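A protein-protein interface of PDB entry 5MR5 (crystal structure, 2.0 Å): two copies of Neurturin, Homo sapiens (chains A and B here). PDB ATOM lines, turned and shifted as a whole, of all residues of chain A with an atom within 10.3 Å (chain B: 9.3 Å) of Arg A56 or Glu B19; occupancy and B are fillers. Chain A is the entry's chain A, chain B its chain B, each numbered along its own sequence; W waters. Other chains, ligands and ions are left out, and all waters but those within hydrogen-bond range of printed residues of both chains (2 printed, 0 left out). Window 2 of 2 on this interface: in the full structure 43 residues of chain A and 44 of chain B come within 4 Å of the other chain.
Of chain A, only Arg A52, Leu A53, Arg A56 and Arg A58 come within 4 Å of Glu B19. No residue of chain A comes within 4 Å of Ser B18. Leu B20 touches just these residues of chain A: Arg A52 (3.6 Å) and Leu A53 (3.9 Å). Of the printed residues of chain A, Glu B14 touches Arg A58 (2.9 Å). Printed residues of chain A within 4 Å of Gly B21: Arg A52 (3.5 Å). Val A64 touches none of the printed residues of chain B. Thr B29 touches none of the printed residues of chain A. The nearest residue of chain B that does not touch Arg A56 is Ser B18 (5.6 Å). The nearest residue of chain A that does not touch Glu B19 is Gly A49 (6.1 Å). The nearest printed residue of chain B that does not touch Leu A59 is Phe B32 (6.1 Å).
O of Glu B19 lies within hydrogen-bond range of NH1 of Arg A52 (2.9 Å). The guanidinium group (NH1) of Arg A58 lies within hydrogen-bond range of the backbone carbonyl oxygen (O) of Glu B14 (2.9 Å). The guanidinium group of Arg A58 lies within salt-bridge range of the side-chain carboxylate of Glu B19, at 2.4 Å. NH1 of Arg A52 sits close to N of Gly B21 (3.5 Å).
No position is printed for both chains. Of the 15 pairs that touch across the chains among the printed residues, none has its exchanged pair printed and touching as well.
Hydrophobic or aromatic side chains of chain B within 4 Å of the printed part of chain A: Leu B13, Val B15, Leu B20, Leu B22 and Phe B32. Of the 16 printed residues of chain A, 7 touch a printed residue of chain B. Among the printed residues, 15 pairs touch across the chains.
The backbone carbonyl oxygen (O) of Leu A53 is in hydrogen-bond range of the backbone NH (N) of Arg A58, at 3.0 Å. The backbone carbonyl oxygen (O) of Leu B13 sits at hydrogen-bond distance from the backbone NH (N) of Phe B32 (2.7 Å). The backbone NH (N) of Val B30 sits at hydrogen-bond distance from the backbone carbonyl oxygen (O) of Val B15 (2.8 Å). The backbone NH (N) of Arg B16 sits at hydrogen-bond distance from the side-chain carboxylate (OE2) of Glu B19, 3.2 Å away.
Water W2 lies within hydrogen-bond range of NH1 of Arg A56 (2.8 Å) and OE1 of Glu B19 (3.0 Å). Water W1 lies within hydrogen-bond range of O of Ser B18, NH1 of Arg A52 and NH2 of Arg A56.
Among the printed residues, pairs that only touch across the chains: Leu A48 with Leu B22, Leu A50 with Phe B32, Arg A52 with Leu B20, Leu A53 with Val B15, Leu A53 with Glu B19, Leu A53 with Leu B20, Leu A53 with Phe B32, Arg A56 with Glu B19, Arg A58 with Leu B13, Arg A58 with Val B15 and Leu A59 with Leu B13.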
ATOM      1  N   VAL A  45       8.493 -16.343  22.112  1.00  0.00           N
ATOM      2  CA  VAL A  45       7.939 -17.415  22.947  1.00  0.00           C
ATOM      3  C   VAL A  45       6.995 -16.872  24.027  1.00  0.00           C
ATOM      4  O   VAL A  45       5.980 -17.479  24.327  1.00  0.00           O
ATOM      5  CB  VAL A  45       9.021 -18.348  23.558  1.00  0.00           C
ATOM      6  CG1 VAL A  45       9.741 -19.073  22.445  1.00  0.00           C
ATOM      7  CG2 VAL A  45      10.013 -17.594  24.429  1.00  0.00           C
ATOM      8  N   LEU A  48       3.645 -16.390  22.372  1.00  0.00           N
ATOM      9  CA  LEU A  48       3.041 -17.677  22.085  1.00  0.00           C
ATOM     10  C   LEU A  48       2.456 -18.267  23.360  1.00  0.00           C
ATOM     11  O   LEU A  48       1.337 -18.760  23.362  1.00  0.00           O
ATOM     12  CB  LEU A  48       4.077 -18.622  21.469  1.00  0.00           C
ATOM     13  CG  LEU A  48       4.177 -18.799  19.941  1.00  0.00           C
ATOM     14  CD1 LEU A  48       3.302 -17.884  19.117  1.00  0.00           C
ATOM     15  CD2 LEU A  48       5.626 -18.738  19.484  1.00  0.00           C
ATOM     16  N   GLY A  49       3.207 -18.189  24.448  1.00  0.00           N
ATOM     17  CA  GLY A  49       2.736 -18.680  25.733  1.00  0.00           C
ATOM     18  C   GLY A  49       1.536 -17.920  26.248  1.00  0.00           C
ATOM     19  O   GLY A  49       0.605 -18.504  26.799  1.00  0.00           O
ATOM     20  N   LEU A  50       1.558 -16.611  26.072  1.00  0.00           N
ATOM     21  CA  LEU A  50       0.471 -15.763  26.507  1.00  0.00           C
ATOM     22  C   LEU A  50      -0.797 -16.046  25.695  1.00  0.00           C
ATOM     23  O   LEU A  50      -1.874 -16.163  26.263  1.00  0.00           O
ATOM     24  CB  LEU A  50       0.893 -14.291  26.376  1.00  0.00           C
ATOM     25  CG  LEU A  50       0.171 -13.180  27.098  1.00  0.00           C
ATOM     26  CD1 LEU A  50       0.013 -13.465  28.591  1.00  0.00           C
ATOM     27  CD2 LEU A  50       0.933 -11.874  26.861  1.00  0.00           C
ATOM     28  N   ARG A  51      -0.685 -16.172  24.378  1.00  0.00           N
ATOM     29  CA  ARG A  51      -1.856 -16.529  23.556  1.00  0.00           C
ATOM     30  C   ARG A  51      -2.481 -17.834  24.006  1.00  0.00           C
ATOM     31  O   ARG A  51      -3.706 -17.929  24.141  1.00  0.00           O
ATOM     32  CB  ARG A  51      -1.491 -16.674  22.085  1.00  0.00           C
ATOM     33  CG  ARG A  51      -1.448 -15.356  21.348  1.00  0.00           C
ATOM     34  CD  ARG A  51      -0.752 -15.461  19.996  1.00  0.00           C
ATOM     35  NE  ARG A  51       0.062 -14.279  19.736  1.00  0.00           N
ATOM     36  CZ  ARG A  51       0.861 -14.115  18.684  1.00  0.00           C
ATOM     37  NH1 ARG A  51       0.969 -15.057  17.755  1.00  0.00           N
ATOM     38  NH2 ARG A  51       1.545 -12.987  18.559  1.00  0.00           N
ATOM     39  N   ARG A  52      -1.640 -18.841  24.237  1.00  0.00           N
ATOM     40  CA  ARG A  52      -2.129 -20.137  24.659  1.00  0.00           C
ATOM     41  C   ARG A  52      -2.860 -20.025  26.000  1.00  0.00           C
ATOM     42  O   ARG A  52      -3.928 -20.617  26.187  1.00  0.00           O
ATOM     43  CB  ARG A  52      -0.964 -21.142  24.747  1.00  0.00           C
ATOM     44  CG  ARG A  52      -1.309 -22.443  25.453  1.00  0.00           C
ATOM     45  CD  ARG A  52      -2.424 -23.230  24.769  1.00  0.00           C
ATOM     46  NE  ARG A  52      -2.011 -24.127  23.676  1.00  0.00           N
ATOM     47  CZ  ARG A  52      -1.515 -25.368  23.827  1.00  0.00           C
ATOM     48  NH1 ARG A  52      -1.259 -25.891  25.030  1.00  0.00           N
ATOM     49  NH2 ARG A  52      -1.273 -26.111  22.759  1.00  0.00           N
ATOM     50  N   LEU A  53      -2.287 -19.276  26.930  1.00  0.00           N
ATOM     51  CA  LEU A  53      -2.863 -19.171  28.277  1.00  0.00           C
ATOM     52  C   LEU A  53      -4.181 -18.403  28.244  1.00  0.00           C
ATOM     53  O   LEU A  53      -5.125 -18.744  28.949  1.00  0.00           O
ATOM     54  CB  LEU A  53      -1.898 -18.492  29.226  1.00  0.00           C
ATOM     55  CG  LEU A  53      -0.694 -19.314  29.632  1.00  0.00           C
ATOM     56  CD1 LEU A  53       0.324 -18.410  30.280  1.00  0.00           C
ATOM     57  CD2 LEU A  53      -1.123 -20.425  30.591  1.00  0.00           C
ATOM     58  N   ARG A  54      -4.246 -17.375  27.407  1.00  0.00           N
ATOM     59  CA  ARG A  54      -5.501 -16.668  27.166  1.00  0.00           C
ATOM     60  C   ARG A  54      -6.569 -17.634  26.644  1.00  0.00           C
ATOM     61  O   ARG A  54      -7.654 -17.699  27.198  1.00  0.00           O
ATOM     62  CB  ARG A  54      -5.290 -15.515  26.188  1.00  0.00           C
ATOM     63  CG  ARG A  54      -6.525 -14.642  25.973  1.00  0.00           C
ATOM     64  CD  ARG A  54      -6.485 -13.943  24.625  1.00  0.00           C
ATOM     65  NE  ARG A  54      -5.645 -12.755  24.628  1.00  0.00           N
ATOM     66  CZ  ARG A  54      -4.903 -12.319  23.609  1.00  0.00           C
ATOM     67  NH1 ARG A  54      -4.808 -12.992  22.469  1.00  0.00           N
ATOM     68  NH2 ARG A  54      -4.213 -11.203  23.759  1.00  0.00           N
ATOM     69  N   GLN A  55      -6.239 -18.399  25.607  1.00  0.00           N
ATOM     70  CA  GLN A  55      -7.165 -19.358  24.979  1.00  0.00           C
ATOM     71  C   GLN A  55      -7.612 -20.466  25.917  1.00  0.00           C
ATOM     72  O   GLN A  55      -8.709 -21.000  25.758  1.00  0.00           O
ATOM     73  CB  GLN A  55      -6.536 -20.010  23.748  1.00  0.00           C
ATOM     74  CG  GLN A  55      -6.255 -19.051  22.593  1.00  0.00           C
ATOM     75  CD  GLN A  55      -5.266 -19.595  21.553  1.00  0.00           C
ATOM     76  OE1 GLN A  55      -4.462 -20.492  21.837  1.00  0.00           O
ATOM     77  NE2 GLN A  55      -5.321 -19.043  20.338  1.00  0.00           N
ATOM     78  N   ARG A  56      -6.768 -20.827  26.886  1.00  0.00           N
ATOM     79  CA  ARG A  56      -7.109 -21.864  27.859  1.00  0.00           C
ATOM     80  C   ARG A  56      -7.854 -21.259  29.047  1.00  0.00           C
ATOM     81  O   ARG A  56      -8.004 -21.921  30.084  1.00  0.00           O
ATOM     82  CB  ARG A  56      -5.843 -22.611  28.323  1.00  0.00           C
ATOM     83  CG  ARG A  56      -5.221 -23.504  27.244  1.00  0.00           C
ATOM     84  CD  ARG A  56      -5.876 -24.868  27.186  1.00  0.00           C
ATOM     85  NE  ARG A  56      -5.411 -25.647  28.312  1.00  0.00           N
ATOM     86  CZ  ARG A  56      -4.367 -26.464  28.305  1.00  0.00           C
ATOM     87  NH1 ARG A  56      -4.036 -27.083  29.427  1.00  0.00           N
ATOM     88  NH2 ARG A  56      -3.662 -26.680  27.194  1.00  0.00           N
ATOM     89  N   ARG A  57      -8.307 -20.004  28.887  1.00  0.00           N
ATOM     90  CA  ARG A  57      -9.034 -19.261  29.922  1.00  0.00           C
ATOM     91  C   ARG A  57      -8.309 -19.242  31.294  1.00  0.00           C
ATOM     92  O   ARG A  57      -8.939 -19.266  32.363  1.00  0.00           O
ATOM     93  CB  ARG A  57     -10.470 -19.816  30.024  1.00  0.00           C
ATOM     94  CG  ARG A  57     -11.445 -19.210  29.014  1.00  0.00           C
ATOM     95  CD  ARG A  57     -12.150 -17.991  29.620  1.00  0.00           C
ATOM     96  NE  ARG A  57     -12.704 -17.056  28.628  1.00  0.00           N
ATOM     97  CZ  ARG A  57     -14.002 -16.895  28.335  1.00  0.00           C
ATOM     98  NH1 ARG A  57     -14.948 -17.618  28.938  1.00  0.00           N
ATOM     99  NH2 ARG A  57     -14.365 -15.995  27.418  1.00  0.00           N
ATOM    100  N   ARG A  58      -6.979 -19.187  31.248  1.00  0.00           N
ATOM    101  CA  ARG A  58      -6.153 -19.169  32.446  1.00  0.00           C
ATOM    102  C   ARG A  58      -5.858 -17.764  32.974  1.00  0.00           C
ATOM    103  O   ARG A  58      -5.340 -17.638  34.086  1.00  0.00           O
ATOM    104  CB  ARG A  58      -4.828 -19.886  32.184  1.00  0.00           C
ATOM    105  CG  ARG A  58      -4.970 -21.383  31.976  1.00  0.00           C
ATOM    106  CD  ARG A  58      -5.059 -22.131  33.294  1.00  0.00           C
ATOM    107  NE  ARG A  58      -3.730 -22.498  33.778  1.00  0.00           N
ATOM    108  CZ  ARG A  58      -3.098 -21.981  34.826  1.00  0.00           C
ATOM    109  NH1 ARG A  58      -1.886 -22.432  35.122  1.00  0.00           N
ATOM    110  NH2 ARG A  58      -3.647 -21.034  35.576  1.00  0.00           N
ATOM    111  N   LEU A  59      -6.175 -16.723  32.201  1.00  0.00           N
ATOM    112  CA  LEU A  59      -5.902 -15.320  32.598  1.00  0.00           C
ATOM    113  C   LEU A  59      -7.101 -14.643  33.288  1.00  0.00           C
ATOM    114  O   LEU A  59      -8.168 -15.230  33.367  1.00  0.00           O
ATOM    115  CB  LEU A  59      -5.439 -14.513  31.374  1.00  0.00           C
ATOM    116  CG  LEU A  59      -3.951 -14.595  30.993  1.00  0.00           C
ATOM    117  CD1 LEU A  59      -3.193 -15.710  31.691  1.00  0.00           C
ATOM    118  CD2 LEU A  59      -3.783 -14.704  29.489  1.00  0.00           C
ATOM    119  N   ARG A  60      -6.902 -13.412  33.767  1.00  0.00           N
ATOM    120  CA  ARG A  60      -7.798 -12.757  34.729  1.00  0.00           C
ATOM    121  C   ARG A  60      -8.635 -11.570  34.207  1.00  0.00           C
ATOM    122  O   ARG A  60      -8.553 -10.468  34.761  1.00  0.00           O
ATOM    123  CB  ARG A  60      -6.942 -12.297  35.936  1.00  0.00           C
ATOM    124  CG  ARG A  60      -7.675 -12.105  37.271  1.00  0.00           C
ATOM    125  CD  ARG A  60      -8.604 -13.268  37.646  1.00  0.00           C
ATOM    126  NE  ARG A  60      -9.675 -12.886  38.575  1.00  0.00           N
ATOM    127  CZ  ARG A  60     -10.715 -12.098  38.273  1.00  0.00           C
ATOM    128  NH1 ARG A  60     -10.849 -11.553  37.067  1.00  0.00           N
ATOM    129  NH2 ARG A  60     -11.631 -11.832  39.197  1.00  0.00           N
ATOM    130  N   ARG A  61      -9.454 -11.778  33.172  1.00  0.00           N
ATOM    131  CA  ARG A  61     -10.425 -10.744  32.706  1.00  0.00           C
ATOM    132  C   ARG A  61      -9.848  -9.319  32.507  1.00  0.00           C
ATOM    133  O   ARG A  61     -10.566  -8.331  32.624  1.00  0.00           O
ATOM    134  CB  ARG A  61     -11.627 -10.666  33.678  1.00  0.00           C
ATOM    135  CG  ARG A  61     -12.784 -11.627  33.395  1.00  0.00           C
ATOM    136  CD  ARG A  61     -13.271 -12.312  34.669  1.00  0.00           C
ATOM    137  NE  ARG A  61     -12.279 -13.283  35.140  1.00  0.00           N
ATOM    138  CZ  ARG A  61     -12.420 -14.089  36.190  1.00  0.00           C
ATOM    139  NH1 ARG A  61     -13.527 -14.060  36.925  1.00  0.00           N
ATOM    140  NH2 ARG A  61     -11.436 -14.927  36.513  1.00  0.00           N
ATOM    141  N   VAL A  64      -4.848  -7.926  27.890  1.00  0.00           N
ATOM    142  CA  VAL A  64      -3.487  -8.457  27.747  1.00  0.00           C
ATOM    143  C   VAL A  64      -3.100  -8.432  26.270  1.00  0.00           C
ATOM    144  O   VAL A  64      -3.821  -8.950  25.431  1.00  0.00           O
ATOM    145  CB  VAL A  64      -3.339  -9.897  28.322  1.00  0.00           C
ATOM    146  CG1 VAL A  64      -3.818  -9.945  29.766  1.00  0.00           C
ATOM    147  CG2 VAL A  64      -4.108 -10.928  27.507  1.00  0.00           C
ATOM    148  N   LEU B  13       1.557 -15.865  37.203  1.00  0.00           N
ATOM    149  CA  LEU B  13       0.727 -17.038  37.110  1.00  0.00           C
ATOM    150  C   LEU B  13       1.649 -18.270  37.209  1.00  0.00           C
ATOM    151  O   LEU B  13       2.684 -18.296  36.559  1.00  0.00           O
ATOM    152  CB  LEU B  13       0.033 -17.025  35.741  1.00  0.00           C
ATOM    153  CG  LEU B  13      -1.428 -17.416  35.596  1.00  0.00           C
ATOM    154  CD1 LEU B  13      -1.591 -18.170  34.299  1.00  0.00           C
ATOM    155  CD2 LEU B  13      -1.950 -18.247  36.756  1.00  0.00           C
ATOM    156  N   GLU B  14       1.284 -19.271  38.016  1.00  0.00           N
ATOM    157  CA  GLU B  14       2.013 -20.550  38.034  1.00  0.00           C
ATOM    158  C   GLU B  14       1.484 -21.382  36.908  1.00  0.00           C
ATOM    159  O   GLU B  14       0.284 -21.543  36.810  1.00  0.00           O
ATOM    160  CB  GLU B  14       1.790 -21.301  39.343  1.00  0.00           C
ATOM    161  CG  GLU B  14       2.331 -20.573  40.548  1.00  0.00           C
ATOM    162  CD  GLU B  14       2.129 -21.337  41.847  1.00  0.00           C
ATOM    163  OE1 GLU B  14       2.375 -20.716  42.892  1.00  0.00           O
ATOM    164  OE2 GLU B  14       1.750 -22.529  41.829  1.00  0.00           O
ATOM    165  N   VAL B  15       2.358 -21.874  36.030  1.00  0.00           N
ATOM    166  CA  VAL B  15       1.920 -22.680  34.897  1.00  0.00           C
ATOM    167  C   VAL B  15       2.771 -23.937  34.741  1.00  0.00           C
ATOM    168  O   VAL B  15       3.948 -23.969  35.122  1.00  0.00           O
ATOM    169  CB  VAL B  15       1.938 -21.894  33.571  1.00  0.00           C
ATOM    170  CG1 VAL B  15       1.125 -20.608  33.688  1.00  0.00           C
ATOM    171  CG2 VAL B  15       3.362 -21.569  33.144  1.00  0.00           C
ATOM    172  N   ARG B  16       2.151 -24.964  34.181  1.00  0.00           N
ATOM    173  CA  ARG B  16       2.851 -26.157  33.709  1.00  0.00           C
ATOM    174  C   ARG B  16       3.489 -25.840  32.373  1.00  0.00           C
ATOM    175  O   ARG B  16       2.817 -25.328  31.477  1.00  0.00           O
ATOM    176  CB  ARG B  16       1.869 -27.284  33.432  1.00  0.00           C
ATOM    177  CG  ARG B  16       1.430 -28.215  34.551  1.00  0.00           C
ATOM    178  CD  ARG B  16       2.155 -28.140  35.862  1.00  0.00           C
ATOM    179  NE  ARG B  16       1.381 -28.898  36.856  1.00  0.00           N
ATOM    180  CZ  ARG B  16       1.262 -30.227  36.904  1.00  0.00           C
ATOM    181  NH1 ARG B  16       0.520 -30.789  37.857  1.00  0.00           N
ATOM    182  NH2 ARG B  16       1.874 -31.006  36.020  1.00  0.00           N
ATOM    183  N   VAL B  17       4.754 -26.201  32.200  1.00  0.00           N
ATOM    184  CA  VAL B  17       5.446 -25.955  30.954  1.00  0.00           C
ATOM    185  C   VAL B  17       4.718 -26.569  29.751  1.00  0.00           C
ATOM    186  O   VAL B  17       4.690 -25.993  28.673  1.00  0.00           O
ATOM    187  CB  VAL B  17       6.899 -26.473  31.014  1.00  0.00           C
ATOM    188  CG1 VAL B  17       7.511 -26.507  29.629  1.00  0.00           C
ATOM    189  CG2 VAL B  17       7.733 -25.573  31.917  1.00  0.00           C
ATOM    190  N   SER B  18       4.146 -27.748  29.941  1.00  0.00           N
ATOM    191  CA  SER B  18       3.418 -28.477  28.868  1.00  0.00           C
ATOM    192  C   SER B  18       2.175 -27.755  28.373  1.00  0.00           C
ATOM    193  O   SER B  18       1.761 -27.928  27.231  1.00  0.00           O
ATOM    194  CB  SER B  18       2.980 -29.814  29.425  1.00  0.00           C
ATOM    195  OG  SER B  18       2.238 -29.608  30.598  1.00  0.00           O
ATOM    196  N   GLU B  19       1.615 -26.944  29.261  1.00  0.00           N
ATOM    197  CA  GLU B  19       0.416 -26.148  29.043  1.00  0.00           C
ATOM    198  C   GLU B  19       0.624 -25.026  28.037  1.00  0.00           C
ATOM    199  O   GLU B  19      -0.351 -24.514  27.467  1.00  0.00           O
ATOM    200  CB  GLU B  19       0.077 -25.496  30.390  1.00  0.00           C
ATOM    201  CG  GLU B  19      -1.304 -24.975  30.564  1.00  0.00           C
ATOM    202  CD  GLU B  19      -1.485 -24.262  31.887  1.00  0.00           C
ATOM    203  OE1 GLU B  19      -2.528 -23.623  32.006  1.00  0.00           O
ATOM    204  OE2 GLU B  19      -0.628 -24.332  32.798  1.00  0.00           O
ATOM    205  N   LEU B  20       1.883 -24.612  27.861  1.00  0.00           N
ATOM    206  CA  LEU B  20       2.194 -23.472  26.997  1.00  0.00           C
ATOM    207  C   LEU B  20       2.171 -23.805  25.498  1.00  0.00           C
ATOM    208  O   LEU B  20       2.226 -22.912  24.668  1.00  0.00           O
ATOM    209  CB  LEU B  20       3.553 -22.886  27.368  1.00  0.00           C
ATOM    210  CG  LEU B  20       3.695 -22.419  28.817  1.00  0.00           C
ATOM    211  CD1 LEU B  20       5.081 -21.871  29.093  1.00  0.00           C
ATOM    212  CD2 LEU B  20       2.639 -21.397  29.195  1.00  0.00           C
ATOM    213  N   GLY B  21       2.121 -25.087  25.154  1.00  0.00           N
ATOM    214  CA  GLY B  21       1.980 -25.496  23.751  1.00  0.00           C
ATOM    215  C   GLY B  21       3.230 -25.202  22.925  1.00  0.00           C
ATOM    216  O   GLY B  21       3.135 -24.963  21.714  1.00  0.00           O
ATOM    217  N   LEU B  22       4.385 -25.219  23.587  1.00  0.00           N
ATOM    218  CA  LEU B  22       5.637 -24.850  22.963  1.00  0.00           C
ATOM    219  C   LEU B  22       6.473 -26.063  22.561  1.00  0.00           C
ATOM    220  O   LEU B  22       7.614 -25.912  22.174  1.00  0.00           O
ATOM    221  CB  LEU B  22       6.449 -23.959  23.907  1.00  0.00           C
ATOM    222  CG  LEU B  22       5.899 -22.549  24.141  1.00  0.00           C
ATOM    223  CD1 LEU B  22       6.716 -21.867  25.246  1.00  0.00           C
ATOM    224  CD2 LEU B  22       5.937 -21.725  22.866  1.00  0.00           C
ATOM    225  N   GLY B  23       5.891 -27.260  22.630  1.00  0.00           N
ATOM    226  CA  GLY B  23       6.592 -28.473  22.233  1.00  0.00           C
ATOM    227  C   GLY B  23       7.408 -29.154  23.319  1.00  0.00           C
ATOM    228  O   GLY B  23       8.115 -30.116  23.023  1.00  0.00           O
ATOM    229  N   TYR B  24       7.310 -28.680  24.564  1.00  0.00           N
ATOM    230  CA  TYR B  24       8.019 -29.288  25.681  1.00  0.00           C
ATOM    231  C   TYR B  24       7.112 -30.216  26.454  1.00  0.00           C
ATOM    232  O   TYR B  24       6.125 -29.780  27.045  1.00  0.00           O
ATOM    233  CB  TYR B  24       8.561 -28.225  26.635  1.00  0.00           C
ATOM    234  CG  TYR B  24       9.542 -27.293  25.980  1.00  0.00           C
ATOM    235  CD1 TYR B  24      10.816 -27.744  25.602  1.00  0.00           C
ATOM    236  CD2 TYR B  24       9.205 -25.965  25.734  1.00  0.00           C
ATOM    237  CE1 TYR B  24      11.718 -26.896  24.981  1.00  0.00           C
ATOM    238  CE2 TYR B  24      10.091 -25.113  25.099  1.00  0.00           C
ATOM    239  CZ  TYR B  24      11.343 -25.577  24.725  1.00  0.00           C
ATOM    240  OH  TYR B  24      12.238 -24.723  24.119  1.00  0.00           O
ATOM    241  N   ALA B  25       7.452 -31.491  26.452  1.00  0.00           N
ATOM    242  CA  ALA B  25       6.700 -32.488  27.191  1.00  0.00           C
ATOM    243  C   ALA B  25       7.232 -32.560  28.613  1.00  0.00           C
ATOM    244  O   ALA B  25       7.969 -33.470  28.953  1.00  0.00           O
ATOM    245  CB  ALA B  25       6.822 -33.847  26.500  1.00  0.00           C
ATOM    246  N   SER B  26       6.902 -31.565  29.426  1.00  0.00           N
ATOM    247  CA  SER B  26       7.370 -31.505  30.808  1.00  0.00           C
ATOM    248  C   SER B  26       6.240 -31.138  31.736  1.00  0.00           C
ATOM    249  O   SER B  26       5.526 -30.147  31.504  1.00  0.00           O
ATOM    250  CB  SER B  26       8.504 -30.505  30.956  1.00  0.00           C
ATOM    251  OG  SER B  26       8.870 -30.316  32.334  1.00  0.00           O
ATOM    252  N   ASP B  27       6.091 -31.918  32.803  1.00  0.00           N
ATOM    253  CA  ASP B  27       5.131 -31.590  33.850  1.00  0.00           C
ATOM    254  C   ASP B  27       5.663 -30.554  34.862  1.00  0.00           C
ATOM    255  O   ASP B  27       4.975 -30.267  35.838  1.00  0.00           O
ATOM    256  CB  ASP B  27       4.718 -32.851  34.615  1.00  0.00           C
ATOM    257  CG  ASP B  27       4.013 -33.865  33.746  1.00  0.00           C
ATOM    258  OD1 ASP B  27       3.452 -33.508  32.694  1.00  0.00           O
ATOM    259  OD2 ASP B  27       4.020 -35.050  34.137  1.00  0.00           O
ATOM    260  N   GLU B  28       6.879 -30.023  34.656  1.00  0.00           N
ATOM    261  CA  GLU B  28       7.423 -28.975  35.524  1.00  0.00           C
ATOM    262  C   GLU B  28       6.559 -27.702  35.524  1.00  0.00           C
ATOM    263  O   GLU B  28       5.847 -27.416  34.547  1.00  0.00           O
ATOM    264  CB  GLU B  28       8.860 -28.625  35.147  1.00  0.00           C
ATOM    265  CG  GLU B  28       9.861 -29.668  35.624  1.00  0.00           C
ATOM    266  CD  GLU B  28      11.206 -29.091  36.084  1.00  0.00           C
ATOM    267  OE1 GLU B  28      11.263 -27.926  36.548  1.00  0.00           O
ATOM    268  OE2 GLU B  28      12.222 -29.819  35.978  1.00  0.00           O
ATOM    269  N   THR B  29       6.599 -26.952  36.622  1.00  0.00           N
ATOM    270  CA  THR B  29       5.909 -25.657  36.643  1.00  0.00           C
ATOM    271  C   THR B  29       6.907 -24.499  36.666  1.00  0.00           C
ATOM    272  O   THR B  29       8.002 -24.590  37.229  1.00  0.00           O
ATOM    273  CB  THR B  29       4.768 -25.501  37.718  1.00  0.00           C
ATOM    274  OG1 THR B  29       4.995 -24.393  38.607  1.00  0.00           O
ATOM    275  CG2 THR B  29       4.490 -26.725  38.461  1.00  0.00           C
ATOM    276  N   VAL B  30       6.536 -23.423  35.987  1.00  0.00           N
ATOM    277  CA  VAL B  30       7.314 -22.208  36.025  1.00  0.00           C
ATOM    278  C   VAL B  30       6.418 -21.071  36.468  1.00  0.00           C
ATOM    279  O   VAL B  30       5.202 -21.143  36.320  1.00  0.00           O
ATOM    280  CB  VAL B  30       7.921 -21.863  34.653  1.00  0.00           C
ATOM    281  CG1 VAL B  30       8.827 -22.987  34.184  1.00  0.00           C
ATOM    282  CG2 VAL B  30       6.841 -21.566  33.617  1.00  0.00           C
ATOM    283  N   PHE B  32       5.121 -17.875  35.449  1.00  0.00           N
ATOM    284  CA  PHE B  32       4.996 -17.125  34.216  1.00  0.00           C
ATOM    285  C   PHE B  32       4.610 -15.682  34.542  1.00  0.00           C
ATOM    286  O   PHE B  32       3.565 -15.440  35.124  1.00  0.00           O
ATOM    287  CB  PHE B  32       3.983 -17.775  33.261  1.00  0.00           C
ATOM    288  CG  PHE B  32       3.906 -17.096  31.926  1.00  0.00           C
ATOM    289  CD1 PHE B  32       4.846 -17.351  30.951  1.00  0.00           C
ATOM    290  CD2 PHE B  32       2.921 -16.145  31.663  1.00  0.00           C
ATOM    291  CE1 PHE B  32       4.799 -16.701  29.713  1.00  0.00           C
ATOM    292  CE2 PHE B  32       2.867 -15.502  30.435  1.00  0.00           C
ATOM    293  CZ  PHE B  32       3.808 -15.773  29.461  1.00  0.00           C
HETATM  294  O   HOH W   1      -0.998 -28.549  26.467  1.00  0.00           O
HETATM  295  O   HOH W   2      -4.037 -26.231  32.138  1.00  0.00           O
